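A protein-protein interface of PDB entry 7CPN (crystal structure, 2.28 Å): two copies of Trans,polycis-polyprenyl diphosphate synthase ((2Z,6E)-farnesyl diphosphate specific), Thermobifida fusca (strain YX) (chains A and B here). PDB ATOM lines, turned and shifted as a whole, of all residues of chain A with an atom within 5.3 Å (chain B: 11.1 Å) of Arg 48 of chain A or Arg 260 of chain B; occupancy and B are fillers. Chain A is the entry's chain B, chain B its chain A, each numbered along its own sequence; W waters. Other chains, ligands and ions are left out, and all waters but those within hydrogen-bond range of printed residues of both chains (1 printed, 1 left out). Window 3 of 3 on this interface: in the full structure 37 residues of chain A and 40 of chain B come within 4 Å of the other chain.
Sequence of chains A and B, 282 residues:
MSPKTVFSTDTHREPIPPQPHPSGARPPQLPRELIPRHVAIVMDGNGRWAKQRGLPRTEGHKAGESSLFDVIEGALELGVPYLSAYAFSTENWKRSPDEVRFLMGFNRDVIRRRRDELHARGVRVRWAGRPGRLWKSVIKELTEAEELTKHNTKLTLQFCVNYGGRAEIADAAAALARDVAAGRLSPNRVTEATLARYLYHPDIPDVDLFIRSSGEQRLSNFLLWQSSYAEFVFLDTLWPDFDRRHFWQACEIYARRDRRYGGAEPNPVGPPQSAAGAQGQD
Arg 48 of chain A touches just one residue of chain B: Arg 260 (3.8 Å).
Arg 260 of chain B touches three residues of chain A.
No residue of chain B comes within 4 Å of Ala 50 of chain A.
Gln 52 of chain A touches none of the printed residues of chain B.
No residue of chain B comes within 4 Å of Ser 214 of chain A.
Of the printed residues of chain B, Glu 216 of chain A touches Arg 260.
Of the printed residues of chain A, Asp 258 of chain B touches Arg 218.
Of the printed residues of chain A, Gly 263 of chain B touches Lys 94 (3.9 Å).
Printed residues of chain A within 4 Å of Ala 230 of chain B: Arg 218 (3.3 Å).
Leu 238 of chain A touches none of the printed residues of chain B.
The nearest residue of chain A that does not touch Arg 260 of chain B is Lys 94 of chain A (5.2 Å).
The nearest printed residue of chain B that does not touch Arg 218 of chain A is Arg 259 of chain B (4.2 Å).
NH2 of Arg 260 of chain B touches NH2 of Arg 48 of chain A (3.8 Å).
CB of Lys 94 of chain A touches CA of Gly 263 of chain B, 3.9 Å away.
Arg 218 of chain A touches Ala 230 of chain B.
The side-chain carboxylate (OE2) of Glu 231 of chain B is in salt-bridge range of the guanidinium group (NH2) of Arg 218 of chain A (2.9 Å).
The backbone carbonyl oxygen (O) of Asp 258 of chain B is in hydrogen-bond range of the guanidinium group (NH2) of Arg 218 of chain A (2.8 Å).
The guanidinium group (NH2) of Arg 260 of chain B lies within salt-bridge range of the side-chain carboxylate (OE1) of Glu 216 of chain A, at 2.7 Å.
The side-chain amino group (NZ) of Lys 94 of chain A sits at hydrogen-bond distance from the backbone carbonyl oxygen (O) of Tyr 261 of chain B, 3.0 Å away.
NE of Arg 260 of chain B lies close to NH1 of Arg 218 of chain A (3.4 Å).
Of the 16 printed residues of chain A, 4 touch a printed residue of chain B.
Printed residues of chain A that touch a printed residue of chain B: Arg 48, Lys 94, Glu 216 and Arg 218.
Along chain B the printed residues that touch a printed residue of chain A span positions 230 to 263.
Among the printed residues, 8 pairs touch across the chains.
Among the printed residues, Asp or Glu carboxylates within 4 Å of a Lys or Arg side-chain nitrogen of the other chain: Glu 216 of chain A with Arg 260 of chain B (2.7 Å) and Arg 218 of chain A with Glu 231 of chain B (2.9 Å).
Water W1 lies within hydrogen-bond range of OE1 of Glu 231 of chain B (2.6 Å), OE2 of Glu 216 of chain A (2.9 Å) and NH2 of Arg 218 of chain A (3.3 Å).
No position is printed for both chains.
The backbone carbonyl oxygen of Asp 208 of chain B lies within hydrogen-bond range of the backbone NH of Glu 231 of chain B, at 2.9 Å.
OE1 of Glu 231 of chain B is in salt-bridge range of NH2 of Arg 257 of chain B, at 2.7 Å.
The guanidinium group (NH1) of Arg 259 of chain B is in hydrogen-bond range of the side-chain hydroxyl (OH) of Tyr 261 of chain B.
OE1 of Glu 216 of chain A is in salt-bridge range of NH1 of Arg 48 of chain A (3.6 Å).
The side-chain hydroxyl (OG) of Ser 214 of chain A sits at hydrogen-bond distance from the backbone NH (N) of Glu 216 of chain A (3.2 Å).
NH2 of Arg 218 of chain A lies within salt-bridge range of OE2 of Glu 216 of chain A (3.0 Å).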
ATOM      1  N   ASP A  44       6.222 -20.729  -1.519  1.00  0.00           N
ATOM      2  CA  ASP A  44       6.020 -19.320  -1.900  1.00  0.00           C
ATOM      3  C   ASP A  44       7.366 -18.566  -1.945  1.00  0.00           C
ATOM      4  O   ASP A  44       8.354 -18.981  -1.274  1.00  0.00           O
ATOM      5  CB  ASP A  44       4.965 -18.691  -0.997  1.00  0.00           C
ATOM      6  CG  ASP A  44       5.365 -18.593   0.464  1.00  0.00           C
ATOM      7  OD1 ASP A  44       5.869 -19.595   0.990  1.00  0.00           O
ATOM      8  OD2 ASP A  44       5.117 -17.521   1.077  1.00  0.00           O
ATOM      9  N   GLY A  45       7.366 -17.492  -2.728  1.00  0.00           N
ATOM     10  CA  GLY A  45       8.474 -16.536  -2.867  1.00  0.00           C
ATOM     11  C   GLY A  45       9.251 -16.722  -4.163  1.00  0.00           C
ATOM     12  O   GLY A  45      10.363 -16.195  -4.223  1.00  0.00           O
ATOM     13  N   ASN A  46       8.730 -17.470  -5.134  1.00  0.00           N
ATOM     14  CA  ASN A  46       9.449 -17.773  -6.407  1.00  0.00           C
ATOM     15  C   ASN A  46       9.637 -16.450  -7.169  1.00  0.00           C
ATOM     16  O   ASN A  46      10.770 -16.165  -7.590  1.00  0.00           O
ATOM     17  CB  ASN A  46       8.763 -18.838  -7.268  1.00  0.00           C
ATOM     18  CG  ASN A  46       8.667 -20.185  -6.575  1.00  0.00           C
ATOM     19  OD1 ASN A  46       9.674 -20.848  -6.311  1.00  0.00           O
ATOM     20  ND2 ASN A  46       7.456 -20.610  -6.250  1.00  0.00           N
ATOM     21  N   GLY A  47       8.572 -15.659  -7.289  1.00  0.00           N
ATOM     22  CA  GLY A  47       8.589 -14.330  -7.924  1.00  0.00           C
ATOM     23  C   GLY A  47       9.557 -13.382  -7.238  1.00  0.00           C
ATOM     24  O   GLY A  47      10.467 -12.864  -7.916  1.00  0.00           O
ATOM     25  N   ARG A  48       9.357 -13.157  -5.938  1.00  0.00           N
ATOM     26  CA  ARG A  48      10.159 -12.252  -5.069  1.00  0.00           C
ATOM     27  C   ARG A  48      11.650 -12.625  -5.148  1.00  0.00           C
ATOM     28  O   ARG A  48      12.506 -11.716  -5.113  1.00  0.00           O
ATOM     29  CB  ARG A  48       9.630 -12.361  -3.632  1.00  0.00           C
ATOM     30  CG  ARG A  48      10.258 -11.439  -2.596  1.00  0.00           C
ATOM     31  CD  ARG A  48       9.269 -11.042  -1.481  1.00  0.00           C
ATOM     32  NE  ARG A  48       8.885 -12.061  -0.491  1.00  0.00           N
ATOM     33  CZ  ARG A  48       7.712 -12.721  -0.433  1.00  0.00           C
ATOM     34  NH1 ARG A  48       7.507 -13.612   0.527  1.00  0.00           N
ATOM     35  NH2 ARG A  48       6.761 -12.513  -1.335  1.00  0.00           N
ATOM     36  N   TRP A  49      11.949 -13.920  -5.240  1.00  0.00           N
ATOM     37  CA  TRP A  49      13.325 -14.468  -5.289  1.00  0.00           C
ATOM     38  C   TRP A  49      14.002 -14.019  -6.584  1.00  0.00           C
ATOM     39  O   TRP A  49      15.164 -13.603  -6.530  1.00  0.00           O
ATOM     40  CB  TRP A  49      13.293 -15.989  -5.150  1.00  0.00           C
ATOM     41  CG  TRP A  49      14.607 -16.688  -5.297  1.00  0.00           C
ATOM     42  CD1 TRP A  49      15.462 -17.071  -4.310  1.00  0.00           C
ATOM     43  CD2 TRP A  49      15.180 -17.136  -6.531  1.00  0.00           C
ATOM     44  NE1 TRP A  49      16.543 -17.706  -4.854  1.00  0.00           N
ATOM     45  CE2 TRP A  49      16.401 -17.743  -6.221  1.00  0.00           C
ATOM     46  CE3 TRP A  49      14.803 -17.026  -7.871  1.00  0.00           C
ATOM     47  CZ2 TRP A  49      17.226 -18.292  -7.194  1.00  0.00           C
ATOM     48  CZ3 TRP A  49      15.632 -17.552  -8.834  1.00  0.00           C
ATOM     49  CH2 TRP A  49      16.801 -18.210  -8.494  1.00  0.00           C
ATOM     50  N   ALA A  50      13.290 -14.110  -7.703  1.00  0.00           N
ATOM     51  CA  ALA A  50      13.797 -13.762  -9.043  1.00  0.00           C
ATOM     52  C   ALA A  50      13.999 -12.247  -9.143  1.00  0.00           C
ATOM     53  O   ALA A  50      14.971 -11.827  -9.792  1.00  0.00           O
ATOM     54  CB  ALA A  50      12.856 -14.293 -10.085  1.00  0.00           C
ATOM     55  N   LYS A  51      13.147 -11.461  -8.496  1.00  0.00           N
ATOM     56  CA  LYS A  51      13.240  -9.979  -8.491  1.00  0.00           C
ATOM     57  C   LYS A  51      14.534  -9.564  -7.775  1.00  0.00           C
ATOM     58  O   LYS A  51      15.273  -8.741  -8.343  1.00  0.00           O
ATOM     59  CB  LYS A  51      11.992  -9.340  -7.871  1.00  0.00           C
ATOM     60  CG  LYS A  51      11.468  -8.151  -8.668  1.00  0.00           C
ATOM     61  CD  LYS A  51      10.322  -7.404  -8.012  1.00  0.00           C
ATOM     62  CE  LYS A  51      10.763  -6.135  -7.312  1.00  0.00           C
ATOM     63  NZ  LYS A  51       9.638  -5.187  -7.126  1.00  0.00           N
ATOM     64  N   GLN A  52      14.809 -10.151  -6.609  1.00  0.00           N
ATOM     65  CA  GLN A  52      16.020  -9.902  -5.783  1.00  0.00           C
ATOM     66  C   GLN A  52      17.306 -10.225  -6.562  1.00  0.00           C
ATOM     67  O   GLN A  52      18.369  -9.724  -6.152  1.00  0.00           O
ATOM     68  CB  GLN A  52      15.993 -10.751  -4.510  1.00  0.00           C
ATOM     69  CG  GLN A  52      14.980 -10.270  -3.483  1.00  0.00           C
ATOM     70  CD  GLN A  52      15.039 -11.064  -2.203  1.00  0.00           C
ATOM     71  OE1 GLN A  52      15.795 -12.029  -2.081  1.00  0.00           O
ATOM     72  NE2 GLN A  52      14.249 -10.645  -1.226  1.00  0.00           N
ATOM     73  N   ARG A  57      10.499 -13.740 -13.257  1.00  0.00           N
ATOM     74  CA  ARG A  57       9.673 -14.523 -12.286  1.00  0.00           C
ATOM     75  C   ARG A  57       9.682 -16.014 -12.660  1.00  0.00           C
ATOM     76  O   ARG A  57       9.843 -16.838 -11.775  1.00  0.00           O
ATOM     77  CB  ARG A  57       8.235 -13.991 -12.253  1.00  0.00           C
ATOM     78  CG  ARG A  57       8.076 -12.614 -11.619  1.00  0.00           C
ATOM     79  CD  ARG A  57       6.601 -12.227 -11.443  1.00  0.00           C
ATOM     80  NE  ARG A  57       5.852 -13.182 -10.619  1.00  0.00           N
ATOM     81  CZ  ARG A  57       5.621 -13.056  -9.312  1.00  0.00           C
ATOM     82  NH1 ARG A  57       6.049 -11.997  -8.638  1.00  0.00           N
ATOM     83  NH2 ARG A  57       4.958 -14.005  -8.672  1.00  0.00           N
ATOM     84  N   LYS A  94      -6.216 -15.399 -10.282  1.00  0.00           N
ATOM     85  CA  LYS A  94      -6.195 -13.921 -10.125  1.00  0.00           C
ATOM     86  C   LYS A  94      -4.884 -13.336 -10.651  1.00  0.00           C
ATOM     87  O   LYS A  94      -4.819 -12.099 -10.795  1.00  0.00           O
ATOM     88  CB  LYS A  94      -6.347 -13.515  -8.651  1.00  0.00           C
ATOM     89  CG  LYS A  94      -7.702 -13.806  -8.013  1.00  0.00           C
ATOM     90  CD  LYS A  94      -7.712 -13.533  -6.527  1.00  0.00           C
ATOM     91  CE  LYS A  94      -8.991 -13.968  -5.846  1.00  0.00           C
ATOM     92  NZ  LYS A  94      -8.807 -14.063  -4.367  1.00  0.00           N
ATOM     93  N   SER A 214       8.374 -18.926   3.252  1.00  0.00           N
ATOM     94  CA  SER A 214       8.689 -17.487   3.335  1.00  0.00           C
ATOM     95  C   SER A 214       8.269 -16.921   4.710  1.00  0.00           C
ATOM     96  O   SER A 214       7.850 -17.720   5.599  1.00  0.00           O
ATOM     97  CB  SER A 214       7.967 -16.797   2.248  1.00  0.00           C
ATOM     98  OG  SER A 214       6.625 -16.665   2.696  1.00  0.00           O
ATOM     99  N   GLY A 215       8.342 -15.597   4.891  1.00  0.00           N
ATOM    100  CA  GLY A 215       7.937 -14.930   6.148  1.00  0.00           C
ATOM    101  C   GLY A 215       6.429 -14.701   6.277  1.00  0.00           C
ATOM    102  O   GLY A 215       6.039 -14.158   7.298  1.00  0.00           O
ATOM    103  N   GLU A 216       5.636 -15.039   5.254  1.00  0.00           N
ATOM    104  CA  GLU A 216       4.165 -14.839   5.185  1.00  0.00           C
ATOM    105  C   GLU A 216       3.471 -15.770   6.179  1.00  0.00           C
ATOM    106  O   GLU A 216       3.504 -16.970   5.936  1.00  0.00           O
ATOM    107  CB  GLU A 216       3.655 -15.126   3.764  1.00  0.00           C
ATOM    108  CG  GLU A 216       4.214 -14.174   2.730  1.00  0.00           C
ATOM    109  CD  GLU A 216       4.213 -12.704   3.130  1.00  0.00           C
ATOM    110  OE1 GLU A 216       5.075 -11.963   2.599  1.00  0.00           O
ATOM    111  OE2 GLU A 216       3.363 -12.294   3.966  1.00  0.00           O
ATOM    112  N   ARG A 218       0.444 -17.336   7.285  1.00  0.00           N
ATOM    113  CA  ARG A 218      -0.968 -17.600   6.876  1.00  0.00           C
ATOM    114  C   ARG A 218      -1.085 -18.980   6.226  1.00  0.00           C
ATOM    115  O   ARG A 218      -0.055 -19.542   5.776  1.00  0.00           O
ATOM    116  CB  ARG A 218      -1.532 -16.514   5.943  1.00  0.00           C
ATOM    117  CG  ARG A 218      -0.514 -15.855   5.047  1.00  0.00           C
ATOM    118  CD  ARG A 218      -1.115 -14.771   4.165  1.00  0.00           C
ATOM    119  NE  ARG A 218      -0.327 -14.517   2.950  1.00  0.00           N
ATOM    120  CZ  ARG A 218       0.374 -13.396   2.647  1.00  0.00           C
ATOM    121  NH1 ARG A 218       1.013 -13.323   1.491  1.00  0.00           N
ATOM    122  NH2 ARG A 218       0.425 -12.364   3.479  1.00  0.00           N
ATOM    123  N   LEU A 238      13.075 -18.083   0.947  1.00  0.00           N
ATOM    124  CA  LEU A 238      12.258 -18.117  -0.288  1.00  0.00           C
ATOM    125  C   LEU A 238      12.388 -19.516  -0.881  1.00  0.00           C
ATOM    126  O   LEU A 238      13.428 -20.173  -0.643  1.00  0.00           O
ATOM    127  CB  LEU A 238      12.719 -17.006  -1.221  1.00  0.00           C
ATOM    128  CG  LEU A 238      12.681 -15.604  -0.590  1.00  0.00           C
ATOM    129  CD1 LEU A 238      13.151 -14.536  -1.546  1.00  0.00           C
ATOM    130  CD2 LEU A 238      11.279 -15.278  -0.085  1.00  0.00           C
ATOM    131  N   ASP B 208      -9.745 -11.674   9.522  1.00  0.00           N
ATOM    132  CA  ASP B 208      -8.624 -10.929   8.884  1.00  0.00           C
ATOM    133  C   ASP B 208      -7.354 -11.182   9.671  1.00  0.00           C
ATOM    134  O   ASP B 208      -6.290 -11.313   9.073  1.00  0.00           O
ATOM    135  CB  ASP B 208      -8.936  -9.431   8.856  1.00  0.00           C
ATOM    136  CG  ASP B 208     -10.117  -9.133   7.969  1.00  0.00           C
ATOM    137  OD1 ASP B 208     -10.010  -9.444   6.752  1.00  0.00           O
ATOM    138  OD2 ASP B 208     -11.152  -8.684   8.528  1.00  0.00           O
ATOM    139  N   SER B 228      -9.158 -19.037   6.528  1.00  0.00           N
ATOM    140  CA  SER B 228      -8.473 -19.517   5.307  1.00  0.00           C
ATOM    141  C   SER B 228      -7.401 -18.539   4.823  1.00  0.00           C
ATOM    142  O   SER B 228      -6.333 -19.020   4.380  1.00  0.00           O
ATOM    143  CB  SER B 228      -9.495 -19.703   4.185  1.00  0.00           C
ATOM    144  OG  SER B 228      -8.943 -20.452   3.105  1.00  0.00           O
ATOM    145  N   TYR B 229      -7.704 -17.240   4.818  1.00  0.00           N
ATOM    146  CA  TYR B 229      -6.768 -16.186   4.346  1.00  0.00           C
ATOM    147  C   TYR B 229      -6.394 -15.210   5.470  1.00  0.00           C
ATOM    148  O   TYR B 229      -5.825 -14.169   5.179  1.00  0.00           O
ATOM    149  CB  TYR B 229      -7.338 -15.512   3.096  1.00  0.00           C
ATOM    150  CG  TYR B 229      -6.918 -16.280   1.867  1.00  0.00           C
ATOM    151  CD1 TYR B 229      -5.582 -16.293   1.486  1.00  0.00           C
ATOM    152  CD2 TYR B 229      -7.812 -17.027   1.126  1.00  0.00           C
ATOM    153  CE1 TYR B 229      -5.149 -16.999   0.373  1.00  0.00           C
ATOM    154  CE2 TYR B 229      -7.393 -17.760   0.024  1.00  0.00           C
ATOM    155  CZ  TYR B 229      -6.060 -17.753  -0.354  1.00  0.00           C
ATOM    156  OH  TYR B 229      -5.648 -18.478  -1.447  1.00  0.00           O
ATOM    157  N   ALA B 230      -6.603 -15.583   6.719  1.00  0.00           N
ATOM    158  CA  ALA B 230      -6.276 -14.748   7.894  1.00  0.00           C
ATOM    159  C   ALA B 230      -4.761 -14.592   8.066  1.00  0.00           C
ATOM    160  O   ALA B 230      -4.025 -15.550   7.839  1.00  0.00           O
ATOM    161  CB  ALA B 230      -6.860 -15.340   9.144  1.00  0.00           C
ATOM    162  N   GLU B 231      -4.337 -13.419   8.532  1.00  0.00           N
ATOM    163  CA  GLU B 231      -2.958 -13.167   9.011  1.00  0.00           C
ATOM    164  C   GLU B 231      -2.850 -13.711  10.419  1.00  0.00           C
ATOM    165  O   GLU B 231      -3.723 -13.395  11.233  1.00  0.00           O
ATOM    166  CB  GLU B 231      -2.617 -11.674   8.998  1.00  0.00           C
ATOM    167  CG  GLU B 231      -2.524 -11.068   7.618  1.00  0.00           C
ATOM    168  CD  GLU B 231      -1.399 -11.642   6.750  1.00  0.00           C
ATOM    169  OE1 GLU B 231      -0.364 -12.049   7.335  1.00  0.00           O
ATOM    170  OE2 GLU B 231      -1.586 -11.746   5.492  1.00  0.00           O
ATOM    171  N   TYR B 254      -0.575  -6.298  11.832  1.00  0.00           N
ATOM    172  CA  TYR B 254      -1.525  -6.619  10.730  1.00  0.00           C
ATOM    173  C   TYR B 254      -1.449  -5.539   9.649  1.00  0.00           C
ATOM    174  O   TYR B 254      -1.441  -5.879   8.447  1.00  0.00           O
ATOM    175  CB  TYR B 254      -2.967  -6.760  11.236  1.00  0.00           C
ATOM    176  CG  TYR B 254      -4.015  -6.833  10.155  1.00  0.00           C
ATOM    177  CD1 TYR B 254      -4.298  -8.028   9.494  1.00  0.00           C
ATOM    178  CD2 TYR B 254      -4.701  -5.705   9.754  1.00  0.00           C
ATOM    179  CE1 TYR B 254      -5.226  -8.087   8.467  1.00  0.00           C
ATOM    180  CE2 TYR B 254      -5.636  -5.760   8.739  1.00  0.00           C
ATOM    181  CZ  TYR B 254      -5.902  -6.949   8.089  1.00  0.00           C
ATOM    182  OH  TYR B 254      -6.846  -6.949   7.103  1.00  0.00           O
ATOM    183  N   ARG B 256       0.924  -3.537   8.756  1.00  0.00           N
ATOM    184  CA  ARG B 256       2.161  -3.788   7.950  1.00  0.00           C
ATOM    185  C   ARG B 256       2.130  -5.066   7.057  1.00  0.00           C
ATOM    186  O   ARG B 256       3.024  -5.189   6.183  1.00  0.00           O
ATOM    187  CB  ARG B 256       3.335  -3.836   8.939  1.00  0.00           C
ATOM    188  CG  ARG B 256       3.594  -2.488   9.598  1.00  0.00           C
ATOM    189  CD  ARG B 256       4.914  -2.357  10.329  1.00  0.00           C
ATOM    190  NE  ARG B 256       4.778  -2.605  11.756  1.00  0.00           N
ATOM    191  CZ  ARG B 256       4.937  -3.785  12.353  1.00  0.00           C
ATOM    192  NH1 ARG B 256       5.240  -4.870  11.653  1.00  0.00           N
ATOM    193  NH2 ARG B 256       4.790  -3.870  13.665  1.00  0.00           N
ATOM    194  N   ARG B 257       1.207  -6.024   7.245  1.00  0.00           N
ATOM    195  CA  ARG B 257       1.221  -7.305   6.466  1.00  0.00           C
ATOM    196  C   ARG B 257       0.835  -7.054   5.000  1.00  0.00           C
ATOM    197  O   ARG B 257      -0.017  -6.179   4.743  1.00  0.00           O
ATOM    198  CB  ARG B 257       0.297  -8.366   7.075  1.00  0.00           C
ATOM    199  CG  ARG B 257       0.736  -8.877   8.439  1.00  0.00           C
ATOM    200  CD  ARG B 257       1.926  -9.785   8.331  1.00  0.00           C
ATOM    201  NE  ARG B 257       2.340 -10.273   9.631  1.00  0.00           N
ATOM    202  CZ  ARG B 257       1.828 -11.307  10.275  1.00  0.00           C
ATOM    203  NH1 ARG B 257       2.335 -11.640  11.448  1.00  0.00           N
ATOM    204  NH2 ARG B 257       0.834 -12.018   9.759  1.00  0.00           N
ATOM    205  N   ASP B 258       1.408  -7.839   4.073  1.00  0.00           N
ATOM    206  CA  ASP B 258       1.082  -7.816   2.610  1.00  0.00           C
ATOM    207  C   ASP B 258       0.050  -8.913   2.259  1.00  0.00           C
ATOM    208  O   ASP B 258       0.462 -10.025   1.867  1.00  0.00           O
ATOM    209  CB  ASP B 258       2.360  -7.942   1.762  1.00  0.00           C
ATOM    210  N   ARG B 259      -1.249  -8.598   2.311  1.00  0.00           N
ATOM    211  CA  ARG B 259      -2.359  -9.548   1.993  1.00  0.00           C
ATOM    212  C   ARG B 259      -2.569  -9.662   0.470  1.00  0.00           C
ATOM    213  O   ARG B 259      -2.834  -8.633  -0.162  1.00  0.00           O
ATOM    214  CB  ARG B 259      -3.646  -9.090   2.677  1.00  0.00           C
ATOM    215  CG  ARG B 259      -3.481  -8.811   4.160  1.00  0.00           C
ATOM    216  CD  ARG B 259      -4.832  -8.733   4.857  1.00  0.00           C
ATOM    217  NE  ARG B 259      -5.412 -10.066   5.018  1.00  0.00           N
ATOM    218  CZ  ARG B 259      -6.661 -10.328   5.400  1.00  0.00           C
ATOM    219  NH1 ARG B 259      -7.522  -9.350   5.655  1.00  0.00           N
ATOM    220  NH2 ARG B 259      -7.060 -11.583   5.464  1.00  0.00           N
ATOM    221  N   ARG B 260      -2.503 -10.881  -0.088  1.00  0.00           N
ATOM    222  CA  ARG B 260      -2.496 -11.135  -1.565  1.00  0.00           C
ATOM    223  C   ARG B 260      -3.712 -11.976  -2.001  1.00  0.00           C
ATOM    224  O   ARG B 260      -4.140 -11.819  -3.173  1.00  0.00           O
ATOM    225  CB  ARG B 260      -1.169 -11.792  -1.975  1.00  0.00           C
ATOM    226  CG  ARG B 260       0.003 -10.818  -2.041  1.00  0.00           C
ATOM    227  CD  ARG B 260       1.329 -11.442  -2.446  1.00  0.00           C
ATOM    228  NE  ARG B 260       2.147 -11.736  -1.277  1.00  0.00           N
ATOM    229  CZ  ARG B 260       2.928 -10.863  -0.633  1.00  0.00           C
ATOM    230  NH1 ARG B 260       3.037  -9.605  -1.039  1.00  0.00           N
ATOM    231  NH2 ARG B 260       3.610 -11.261   0.428  1.00  0.00           N
ATOM    232  N   TYR B 261      -4.239 -12.840  -1.119  1.00  0.00           N
ATOM    233  CA  TYR B 261      -5.392 -13.762  -1.376  1.00  0.00           C
ATOM    234  C   TYR B 261      -5.141 -14.607  -2.653  1.00  0.00           C
ATOM    235  O   TYR B 261      -6.142 -14.977  -3.344  1.00  0.00           O
ATOM    236  CB  TYR B 261      -6.724 -12.990  -1.444  1.00  0.00           C
ATOM    237  CG  TYR B 261      -6.940 -11.978  -0.343  1.00  0.00           C
ATOM    238  CD1 TYR B 261      -7.343 -12.370   0.928  1.00  0.00           C
ATOM    239  CD2 TYR B 261      -6.709 -10.624  -0.560  1.00  0.00           C
ATOM    240  CE1 TYR B 261      -7.508 -11.452   1.956  1.00  0.00           C
ATOM    241  CE2 TYR B 261      -6.882  -9.687   0.451  1.00  0.00           C
ATOM    242  CZ  TYR B 261      -7.281 -10.104   1.715  1.00  0.00           C
ATOM    243  OH  TYR B 261      -7.468  -9.191   2.712  1.00  0.00           O
ATOM    244  N   GLY B 262      -3.864 -14.920  -2.959  1.00  0.00           N
ATOM    245  CA  GLY B 262      -3.440 -15.742  -4.116  1.00  0.00           C
ATOM    246  C   GLY B 262      -3.139 -14.950  -5.390  1.00  0.00           C
ATOM    247  O   GLY B 262      -2.621 -15.583  -6.344  1.00  0.00           O
ATOM    248  N   GLY B 263      -3.415 -13.633  -5.404  1.00  0.00           N
ATOM    249  CA  GLY B 263      -3.135 -12.705  -6.526  1.00  0.00           C
ATOM    250  C   GLY B 263      -1.670 -12.319  -6.601  1.00  0.00           C
ATOM    251  O   GLY B 263      -0.950 -12.672  -5.652  1.00  0.00           O
HETATM  252  O   HOH W   1       1.917 -12.954   6.362  1.00  0.00           O
